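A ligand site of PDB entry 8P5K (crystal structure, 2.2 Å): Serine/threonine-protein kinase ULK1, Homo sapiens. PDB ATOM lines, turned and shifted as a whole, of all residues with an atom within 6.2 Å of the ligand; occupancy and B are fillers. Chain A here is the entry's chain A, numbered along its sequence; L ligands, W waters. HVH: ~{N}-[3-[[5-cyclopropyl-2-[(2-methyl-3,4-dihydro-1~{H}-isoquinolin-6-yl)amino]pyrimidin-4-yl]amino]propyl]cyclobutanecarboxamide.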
ATOM      1  N   ILE A  23      25.844 -31.962  -2.877  1.00  0.00           N
ATOM      2  CA  ILE A  23      25.334 -31.119  -3.940  1.00  0.00           C
ATOM      3  C   ILE A  23      26.198 -29.861  -4.088  1.00  0.00           C
ATOM      4  O   ILE A  23      25.991 -29.093  -5.017  1.00  0.00           O
ATOM      5  CB  ILE A  23      23.842 -30.790  -3.701  1.00  0.00           C
ATOM      6  CG1 ILE A  23      23.618 -29.835  -2.523  1.00  0.00           C
ATOM      7  CG2 ILE A  23      23.063 -32.077  -3.521  1.00  0.00           C
ATOM      8  CD1 ILE A  23      22.153 -29.520  -2.230  1.00  0.00           C
ATOM      9  N   GLY A  24      27.144 -29.622  -3.178  1.00  0.00           N
ATOM     10  CA  GLY A  24      27.979 -28.438  -3.287  1.00  0.00           C
ATOM     11  C   GLY A  24      29.192 -28.500  -2.384  1.00  0.00           C
ATOM     12  O   GLY A  24      29.148 -29.161  -1.345  1.00  0.00           O
ATOM     13  N   HIS A  25      30.255 -27.788  -2.776  1.00  0.00           N
ATOM     14  CA  HIS A  25      31.499 -27.795  -2.032  1.00  0.00           C
ATOM     15  C   HIS A  25      32.311 -26.558  -2.411  1.00  0.00           C
ATOM     16  O   HIS A  25      32.318 -26.112  -3.565  1.00  0.00           O
ATOM     17  CB  HIS A  25      32.244 -29.117  -2.233  1.00  0.00           C
ATOM     18  CG  HIS A  25      32.560 -29.430  -3.668  1.00  0.00           C
ATOM     19  ND1 HIS A  25      33.813 -29.401  -4.236  1.00  0.00           N
ATOM     20  CD2 HIS A  25      31.722 -29.801  -4.643  1.00  0.00           C
ATOM     21  CE1 HIS A  25      33.716 -29.750  -5.514  1.00  0.00           C
ATOM     22  NE2 HIS A  25      32.464 -30.013  -5.774  1.00  0.00           N
ATOM     23  N   GLY A  26      32.948 -25.993  -1.392  1.00  0.00           N
ATOM     24  CA  GLY A  26      33.943 -24.951  -1.532  1.00  0.00           C
ATOM     25  C   GLY A  26      34.944 -25.124  -0.398  1.00  0.00           C
ATOM     26  O   GLY A  26      34.848 -26.065   0.388  1.00  0.00           O
ATOM     27  N   ALA A  27      35.893 -24.203  -0.311  1.00  0.00           N
ATOM     28  CA  ALA A  27      36.991 -24.328   0.636  1.00  0.00           C
ATOM     29  C   ALA A  27      36.475 -24.286   2.066  1.00  0.00           C
ATOM     30  O   ALA A  27      37.126 -24.823   2.954  1.00  0.00           O
ATOM     31  CB  ALA A  27      37.985 -23.232   0.363  1.00  0.00           C
ATOM     32  N   PHE A  28      35.326 -23.618   2.296  1.00  0.00           N
ATOM     33  CA  PHE A  28      34.879 -23.371   3.659  1.00  0.00           C
ATOM     34  C   PHE A  28      33.543 -24.032   3.979  1.00  0.00           C
ATOM     35  O   PHE A  28      32.986 -23.776   5.046  1.00  0.00           O
ATOM     36  CB  PHE A  28      34.836 -21.864   3.905  1.00  0.00           C
ATOM     37  CG  PHE A  28      36.137 -21.174   3.565  1.00  0.00           C
ATOM     38  CD1 PHE A  28      37.282 -21.468   4.274  1.00  0.00           C
ATOM     39  CD2 PHE A  28      36.207 -20.284   2.510  1.00  0.00           C
ATOM     40  CE1 PHE A  28      38.500 -20.883   3.935  1.00  0.00           C
ATOM     41  CE2 PHE A  28      37.413 -19.684   2.183  1.00  0.00           C
ATOM     42  CZ  PHE A  28      38.555 -19.988   2.892  1.00  0.00           C
ATOM     43  N   ALA A  29      33.017 -24.855   3.069  1.00  0.00           N
ATOM     44  CA  ALA A  29      31.778 -25.540   3.385  1.00  0.00           C
ATOM     45  C   ALA A  29      31.508 -26.676   2.396  1.00  0.00           C
ATOM     46  O   ALA A  29      31.985 -26.679   1.273  1.00  0.00           O
ATOM     47  CB  ALA A  29      30.630 -24.577   3.371  1.00  0.00           C
ATOM     48  N   VAL A  30      30.681 -27.595   2.856  1.00  0.00           N
ATOM     49  CA  VAL A  30      30.147 -28.677   2.059  1.00  0.00           C
ATOM     50  C   VAL A  30      28.638 -28.666   2.258  1.00  0.00           C
ATOM     51  O   VAL A  30      28.143 -28.351   3.347  1.00  0.00           O
ATOM     52  CB  VAL A  30      30.804 -29.991   2.532  1.00  0.00           C
ATOM     53  CG1 VAL A  30      30.066 -31.202   2.047  1.00  0.00           C
ATOM     54  CG2 VAL A  30      32.259 -30.063   2.112  1.00  0.00           C
ATOM     55  N   VAL A  31      27.896 -29.002   1.211  1.00  0.00           N
ATOM     56  CA  VAL A  31      26.445 -28.942   1.255  1.00  0.00           C
ATOM     57  C   VAL A  31      25.902 -30.300   0.814  1.00  0.00           C
ATOM     58  O   VAL A  31      26.317 -30.828  -0.202  1.00  0.00           O
ATOM     59  CB  VAL A  31      25.868 -27.837   0.356  1.00  0.00           C
ATOM     60  CG1 VAL A  31      24.367 -27.706   0.526  1.00  0.00           C
ATOM     61  CG2 VAL A  31      26.533 -26.496   0.646  1.00  0.00           C
ATOM     62  N   ALA A  45      18.738 -28.355   2.037  1.00  0.00           N
ATOM     63  CA  ALA A  45      20.176 -28.409   1.863  1.00  0.00           C
ATOM     64  C   ALA A  45      20.841 -28.130   3.207  1.00  0.00           C
ATOM     65  O   ALA A  45      20.549 -27.127   3.854  1.00  0.00           O
ATOM     66  CB  ALA A  45      20.607 -27.410   0.804  1.00  0.00           C
ATOM     67  N   VAL A  46      21.753 -29.015   3.598  1.00  0.00           N
ATOM     68  CA  VAL A  46      22.387 -28.927   4.891  1.00  0.00           C
ATOM     69  C   VAL A  46      23.830 -28.554   4.654  1.00  0.00           C
ATOM     70  O   VAL A  46      24.569 -29.322   4.030  1.00  0.00           O
ATOM     71  CB  VAL A  46      22.285 -30.247   5.671  1.00  0.00           C
ATOM     72  CG1 VAL A  46      22.999 -30.145   7.005  1.00  0.00           C
ATOM     73  CG2 VAL A  46      20.833 -30.640   5.887  1.00  0.00           C
ATOM     74  N   LYS A  47      24.200 -27.377   5.157  1.00  0.00           N
ATOM     75  CA  LYS A  47      25.554 -26.888   4.967  1.00  0.00           C
ATOM     76  C   LYS A  47      26.369 -27.174   6.221  1.00  0.00           C
ATOM     77  O   LYS A  47      25.971 -26.809   7.330  1.00  0.00           O
ATOM     78  CB  LYS A  47      25.502 -25.388   4.693  1.00  0.00           C
ATOM     79  CG  LYS A  47      26.810 -24.735   4.279  1.00  0.00           C
ATOM     80  CD  LYS A  47      26.589 -23.286   3.849  1.00  0.00           C
ATOM     81  CE  LYS A  47      27.870 -22.651   3.377  1.00  0.00           C
ATOM     82  NZ  LYS A  47      27.585 -21.307   2.844  1.00  0.00           N
ATOM     83  N   VAL A  77      17.752 -17.637  -0.455  1.00  0.00           N
ATOM     84  CA  VAL A  77      17.565 -18.984   0.056  1.00  0.00           C
ATOM     85  C   VAL A  77      17.271 -18.900   1.546  1.00  0.00           C
ATOM     86  O   VAL A  77      17.940 -18.203   2.287  1.00  0.00           O
ATOM     87  CB  VAL A  77      18.777 -19.889  -0.257  1.00  0.00           C
ATOM     88  CG1 VAL A  77      18.547 -21.333   0.173  1.00  0.00           C
ATOM     89  CG2 VAL A  77      19.115 -19.880  -1.743  1.00  0.00           C
ATOM     90  N   ALA A  78      16.234 -19.625   1.991  1.00  0.00           N
ATOM     91  CA  ALA A  78      15.752 -19.473   3.344  1.00  0.00           C
ATOM     92  C   ALA A  78      16.559 -20.353   4.282  1.00  0.00           C
ATOM     93  O   ALA A  78      17.031 -21.435   3.893  1.00  0.00           O
ATOM     94  CB  ALA A  78      14.289 -19.758   3.429  1.00  0.00           C
ATOM     95  N   MET A  93      18.925 -25.297   5.115  1.00  0.00           N
ATOM     96  CA  MET A  93      18.353 -24.339   4.193  1.00  0.00           C
ATOM     97  C   MET A  93      17.434 -24.962   3.159  1.00  0.00           C
ATOM     98  O   MET A  93      17.446 -26.163   2.915  1.00  0.00           O
ATOM     99  CB  MET A  93      19.509 -23.612   3.538  1.00  0.00           C
ATOM    100  CG  MET A  93      19.913 -22.549   4.538  1.00  0.00           C
ATOM    101  SD  MET A  93      21.351 -21.737   4.209  1.00  0.00           S
ATOM    102  CE  MET A  93      22.374 -23.086   3.630  1.00  0.00           C
ATOM    103  N   GLU A  94      16.612 -24.057   2.596  1.00  0.00           N
ATOM    104  CA  GLU A  94      15.833 -24.280   1.401  1.00  0.00           C
ATOM    105  C   GLU A  94      16.663 -25.023   0.349  1.00  0.00           C
ATOM    106  O   GLU A  94      17.826 -24.685   0.124  1.00  0.00           O
ATOM    107  CB  GLU A  94      15.322 -22.928   0.945  1.00  0.00           C
ATOM    108  CG  GLU A  94      14.563 -22.955  -0.342  1.00  0.00           C
ATOM    109  CD  GLU A  94      14.158 -21.580  -0.854  1.00  0.00           C
ATOM    110  OE1 GLU A  94      14.494 -20.541  -0.201  1.00  0.00           O
ATOM    111  OE2 GLU A  94      13.446 -21.551  -1.864  1.00  0.00           O
ATOM    112  N   TYR A  95      16.081 -26.100  -0.204  1.00  0.00           N
ATOM    113  CA  TYR A  95      16.647 -26.796  -1.349  1.00  0.00           C
ATOM    114  C   TYR A  95      16.117 -26.177  -2.631  1.00  0.00           C
ATOM    115  O   TYR A  95      14.914 -25.930  -2.785  1.00  0.00           O
ATOM    116  CB  TYR A  95      16.286 -28.284  -1.334  1.00  0.00           C
ATOM    117  CG  TYR A  95      16.760 -29.053  -2.532  1.00  0.00           C
ATOM    118  CD1 TYR A  95      18.112 -29.294  -2.713  1.00  0.00           C
ATOM    119  CD2 TYR A  95      15.881 -29.538  -3.502  1.00  0.00           C
ATOM    120  CE1 TYR A  95      18.584 -29.995  -3.810  1.00  0.00           C
ATOM    121  CE2 TYR A  95      16.336 -30.246  -4.599  1.00  0.00           C
ATOM    122  CZ  TYR A  95      17.694 -30.456  -4.768  1.00  0.00           C
ATOM    123  OH  TYR A  95      18.138 -31.161  -5.881  1.00  0.00           O
ATOM    124  N   CYS A  96      17.040 -25.852  -3.539  1.00  0.00           N
ATOM    125  CA  CYS A  96      16.666 -25.292  -4.838  1.00  0.00           C
ATOM    126  C   CYS A  96      16.789 -26.401  -5.877  1.00  0.00           C
ATOM    127  O   CYS A  96      17.896 -26.906  -6.117  1.00  0.00           O
ATOM    128  CB  CYS A  96      17.529 -24.055  -5.155  1.00  0.00           C
ATOM    129  SG  CYS A  96      17.190 -22.692  -4.000  1.00  0.00           S
ATOM    130  N   ASN A  97      15.641 -26.828  -6.421  1.00  0.00           N
ATOM    131  CA  ASN A  97      15.634 -28.056  -7.206  1.00  0.00           C
ATOM    132  C   ASN A  97      16.201 -27.840  -8.617  1.00  0.00           C
ATOM    133  O   ASN A  97      16.444 -28.823  -9.299  1.00  0.00           O
ATOM    134  CB  ASN A  97      14.250 -28.709  -7.284  1.00  0.00           C
ATOM    135  CG  ASN A  97      13.208 -27.818  -7.931  1.00  0.00           C
ATOM    136  OD1 ASN A  97      13.505 -26.790  -8.520  1.00  0.00           O
ATOM    137  ND2 ASN A  97      11.963 -28.214  -7.817  1.00  0.00           N
ATOM    138  N   GLY A  98      16.466 -26.578  -9.021  1.00  0.00           N
ATOM    139  CA  GLY A  98      16.948 -26.287 -10.367  1.00  0.00           C
ATOM    140  C   GLY A  98      18.469 -26.245 -10.491  1.00  0.00           C
ATOM    141  O   GLY A  98      18.978 -25.997 -11.582  1.00  0.00           O
ATOM    142  N   GLY A  99      19.203 -26.450  -9.394  1.00  0.00           N
ATOM    143  CA  GLY A  99      20.650 -26.229  -9.397  1.00  0.00           C
ATOM    144  C   GLY A  99      20.998 -24.735  -9.541  1.00  0.00           C
ATOM    145  O   GLY A  99      20.218 -23.857  -9.165  1.00  0.00           O
ATOM    146  N   ASP A 100      22.218 -24.467 -10.025  1.00  0.00           N
ATOM    147  CA  ASP A 100      22.764 -23.125 -10.039  1.00  0.00           C
ATOM    148  C   ASP A 100      22.711 -22.525 -11.446  1.00  0.00           C
ATOM    149  O   ASP A 100      22.509 -23.225 -12.456  1.00  0.00           O
ATOM    150  CB  ASP A 100      24.164 -23.095  -9.439  1.00  0.00           C
ATOM    151  CG  ASP A 100      25.267 -23.746 -10.260  1.00  0.00           C
ATOM    152  OD1 ASP A 100      25.000 -24.130 -11.408  1.00  0.00           O
ATOM    153  OD2 ASP A 100      26.397 -23.902  -9.728  1.00  0.00           O
ATOM    154  N   ASP A 103      25.376 -23.831 -14.133  1.00  0.00           N
ATOM    155  CA  ASP A 103      25.038 -25.049 -14.872  1.00  0.00           C
ATOM    156  C   ASP A 103      23.996 -24.739 -15.942  1.00  0.00           C
ATOM    157  O   ASP A 103      24.111 -25.222 -17.047  1.00  0.00           O
ATOM    158  CB  ASP A 103      24.517 -26.160 -13.962  1.00  0.00           C
ATOM    159  CG  ASP A 103      25.596 -26.778 -13.078  1.00  0.00           C
ATOM    160  OD1 ASP A 103      26.793 -26.704 -13.441  1.00  0.00           O
ATOM    161  OD2 ASP A 103      25.258 -27.316 -12.033  1.00  0.00           O
ATOM    162  N   GLN A 143      27.479 -19.419  -9.637  1.00  0.00           N
ATOM    163  CA  GLN A 143      27.484 -20.585  -8.780  1.00  0.00           C
ATOM    164  C   GLN A 143      26.642 -20.332  -7.526  1.00  0.00           C
ATOM    165  O   GLN A 143      26.220 -21.296  -6.868  1.00  0.00           O
ATOM    166  CB  GLN A 143      28.912 -20.975  -8.387  1.00  0.00           C
ATOM    167  CG  GLN A 143      29.824 -21.414  -9.541  1.00  0.00           C
ATOM    168  CD  GLN A 143      30.277 -20.343 -10.518  1.00  0.00           C
ATOM    169  OE1 GLN A 143      30.184 -19.135 -10.310  1.00  0.00           O
ATOM    170  NE2 GLN A 143      30.781 -20.777 -11.668  1.00  0.00           N
ATOM    171  N   ASN A 144      26.346 -19.059  -7.200  1.00  0.00           N
ATOM    172  CA  ASN A 144      25.634 -18.705  -5.984  1.00  0.00           C
ATOM    173  C   ASN A 144      24.278 -18.090  -6.289  1.00  0.00           C
ATOM    174  O   ASN A 144      23.634 -17.535  -5.397  1.00  0.00           O
ATOM    175  CB  ASN A 144      26.434 -17.715  -5.141  1.00  0.00           C
ATOM    176  CG  ASN A 144      27.585 -18.391  -4.437  1.00  0.00           C
ATOM    177  OD1 ASN A 144      27.589 -19.607  -4.253  1.00  0.00           O
ATOM    178  ND2 ASN A 144      28.568 -17.615  -4.050  1.00  0.00           N
ATOM    179  N   LEU A 146      20.793 -19.559  -7.425  1.00  0.00           N
ATOM    180  CA  LEU A 146      20.168 -20.870  -7.564  1.00  0.00           C
ATOM    181  C   LEU A 146      18.782 -20.749  -8.167  1.00  0.00           C
ATOM    182  O   LEU A 146      18.128 -19.700  -8.049  1.00  0.00           O
ATOM    183  CB  LEU A 146      20.100 -21.536  -6.185  1.00  0.00           C
ATOM    184  CG  LEU A 146      21.449 -21.684  -5.504  1.00  0.00           C
ATOM    185  CD1 LEU A 146      21.324 -22.476  -4.213  1.00  0.00           C
ATOM    186  CD2 LEU A 146      22.478 -22.304  -6.455  1.00  0.00           C
ATOM    187  N   ALA A 165      22.268 -17.290  -2.880  1.00  0.00           N
ATOM    188  CA  ALA A 165      22.784 -18.157  -1.850  1.00  0.00           C
ATOM    189  C   ALA A 165      24.179 -17.723  -1.412  1.00  0.00           C
ATOM    190  O   ALA A 165      24.817 -16.882  -2.039  1.00  0.00           O
ATOM    191  CB  ALA A 165      22.854 -19.583  -2.363  1.00  0.00           C
ATOM    192  N   ASP A 166      24.647 -18.371  -0.354  1.00  0.00           N
ATOM    193  CA  ASP A 166      26.024 -18.342   0.122  1.00  0.00           C
ATOM    194  C   ASP A 166      26.396 -16.948   0.665  1.00  0.00           C
ATOM    195  O   ASP A 166      27.079 -16.181   0.005  1.00  0.00           O
ATOM    196  CB  ASP A 166      27.018 -18.895  -0.894  1.00  0.00           C
ATOM    197  CG  ASP A 166      28.356 -19.198  -0.238  1.00  0.00           C
ATOM    198  OD1 ASP A 166      28.485 -18.962   0.987  1.00  0.00           O
ATOM    199  OD2 ASP A 166      29.282 -19.645  -0.956  1.00  0.00           O
HETATM  200  N1  HVH L   1      24.031 -25.312  -2.384  1.00  0.00           N
HETATM  201  C2  HVH L   1      29.163 -24.477  -2.012  1.00  0.00           C
HETATM  202  N3  HVH L   1      20.580 -27.165  -4.868  1.00  0.00           N
HETATM  203  C4  HVH L   1      28.564 -23.427  -0.229  1.00  0.00           C
HETATM  204  N4  HVH L   1      24.507 -29.375  -9.601  1.00  0.00           N
HETATM  205  C5  HVH L   1      25.426 -23.454  -4.198  1.00  0.00           C
HETATM  206  C6  HVH L   1      25.147 -24.910  -4.527  1.00  0.00           C
HETATM  207  O   HVH L   1      25.951 -23.159  -1.379  1.00  0.00           O
HETATM  208  C   HVH L   1      26.878 -23.241  -2.190  1.00  0.00           C
HETATM  209  C1  HVH L   1      28.323 -23.209  -1.729  1.00  0.00           C
HETATM  210  C3  HVH L   1      29.750 -24.319  -0.608  1.00  0.00           C
HETATM  211  N   HVH L   1      26.707 -23.298  -3.513  1.00  0.00           N
HETATM  212  C7  HVH L   1      25.080 -25.789  -3.280  1.00  0.00           C
HETATM  213  C8  HVH L   1      22.734 -25.480  -2.621  1.00  0.00           C
HETATM  214  C21 HVH L   1      21.812 -24.792  -1.836  1.00  0.00           C
HETATM  215  C22 HVH L   1      22.292 -23.828  -0.807  1.00  0.00           C
HETATM  216  C24 HVH L   1      21.446 -23.395   0.333  1.00  0.00           C
HETATM  217  C23 HVH L   1      22.646 -24.214   0.568  1.00  0.00           C
HETATM  218  C20 HVH L   1      20.478 -24.985  -2.124  1.00  0.00           C
HETATM  219  N5  HVH L   1      20.072 -25.769  -3.126  1.00  0.00           N
HETATM  220  C9  HVH L   1      21.021 -26.378  -3.857  1.00  0.00           C
HETATM  221  N2  HVH L   1      22.338 -26.238  -3.652  1.00  0.00           N
HETATM  222  C10 HVH L   1      21.249 -27.819  -5.936  1.00  0.00           C
HETATM  223  C19 HVH L   1      20.586 -28.825  -6.658  1.00  0.00           C
HETATM  224  C18 HVH L   1      21.207 -29.487  -7.701  1.00  0.00           C
HETATM  225  C13 HVH L   1      22.516 -29.181  -8.058  1.00  0.00           C
HETATM  226  C14 HVH L   1      23.171 -29.928  -9.191  1.00  0.00           C
HETATM  227  C15 HVH L   1      25.272 -30.354 -10.377  1.00  0.00           C
HETATM  228  C16 HVH L   1      25.304 -28.932  -8.443  1.00  0.00           C
HETATM  229  C17 HVH L   1      24.613 -27.808  -7.708  1.00  0.00           C
HETATM  230  C12 HVH L   1      23.198 -28.190  -7.340  1.00  0.00           C
HETATM  231  C11 HVH L   1      22.559 -27.534  -6.284  1.00  0.00           C
HETATM  232  O   HOH W   1      25.399 -21.501   0.780  1.00  0.00           O
HETATM  233  O   HOH W   2      27.703 -27.439  -7.276  1.00  0.00           O
HETATM  234  O   HOH W   3      27.079 -23.810  -7.099  1.00  0.00           O
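Residues that only touch the ligand: Ile 23, Gly 24, His 25, Gly 26, Ala 29, Val 31, Ala 45, Lys 47, Val 77, Met 93, Glu 94, Tyr 95, Gly 99, Gln 143, Asn 144, Leu 146 and Asp 166. 19 residues have an atom within 4 Å of the ligand: Ile 23, Gly 24, His 25, Gly 26, Ala 29, Val 31, Ala 45, Lys 47, Val 77, Met 93, Glu 94, Tyr 95, Cys 96, Gly 99, Asp 103, Gln 143, Asn 144, Leu 146 and Asp 166.
Water W1 lies within hydrogen-bond range of O of the ligand (2.8 Å), NZ of Lys 47 (3.0 Å) and N of Asp 166 (3.4 Å). Water W3 bridges O of Gln 143 (2.7 Å) and OD2 of Asp 100 (2.7 Å).
The side-chain carboxylate of Asp 100 sits at hydrogen-bond distance from the backbone NH of Asp 103, 2.8 Å away. The backbone NH (N) of Ala 45 sits at hydrogen-bond distance from the backbone carbonyl oxygen (O) of Met 93 (2.7 Å). N of Ile 23 is in hydrogen-bond range of O of Val 31. The backbone NH (N) of Ala 78 sits at hydrogen-bond distance from the side-chain carboxylate (OE1) of Glu 94 (2.9 Å). The side-chain amino group of Lys 47 lies within salt-bridge range of the side-chain carboxylate of Asp 166 (3.1 Å). The backbone carbonyl oxygen (O) of Gly 24 is in hydrogen-bond range of the backbone NH (N) of Val 31. O of Asn 144 lies within hydrogen-bond range of N of Ala 165 (2.9 Å).
The backbone NH (N) of Cys 96 is in hydrogen-bond range of a nitrogen (N5) of the ligand. A nitrogen (N3) of the ligand lies within hydrogen-bond range of the backbone carbonyl oxygen (O) of Cys 96. The side-chain carboxylate (OD2) of Asp 103 lies within salt-bridge range of a nitrogen (N4) of the ligand (3.3 Å).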
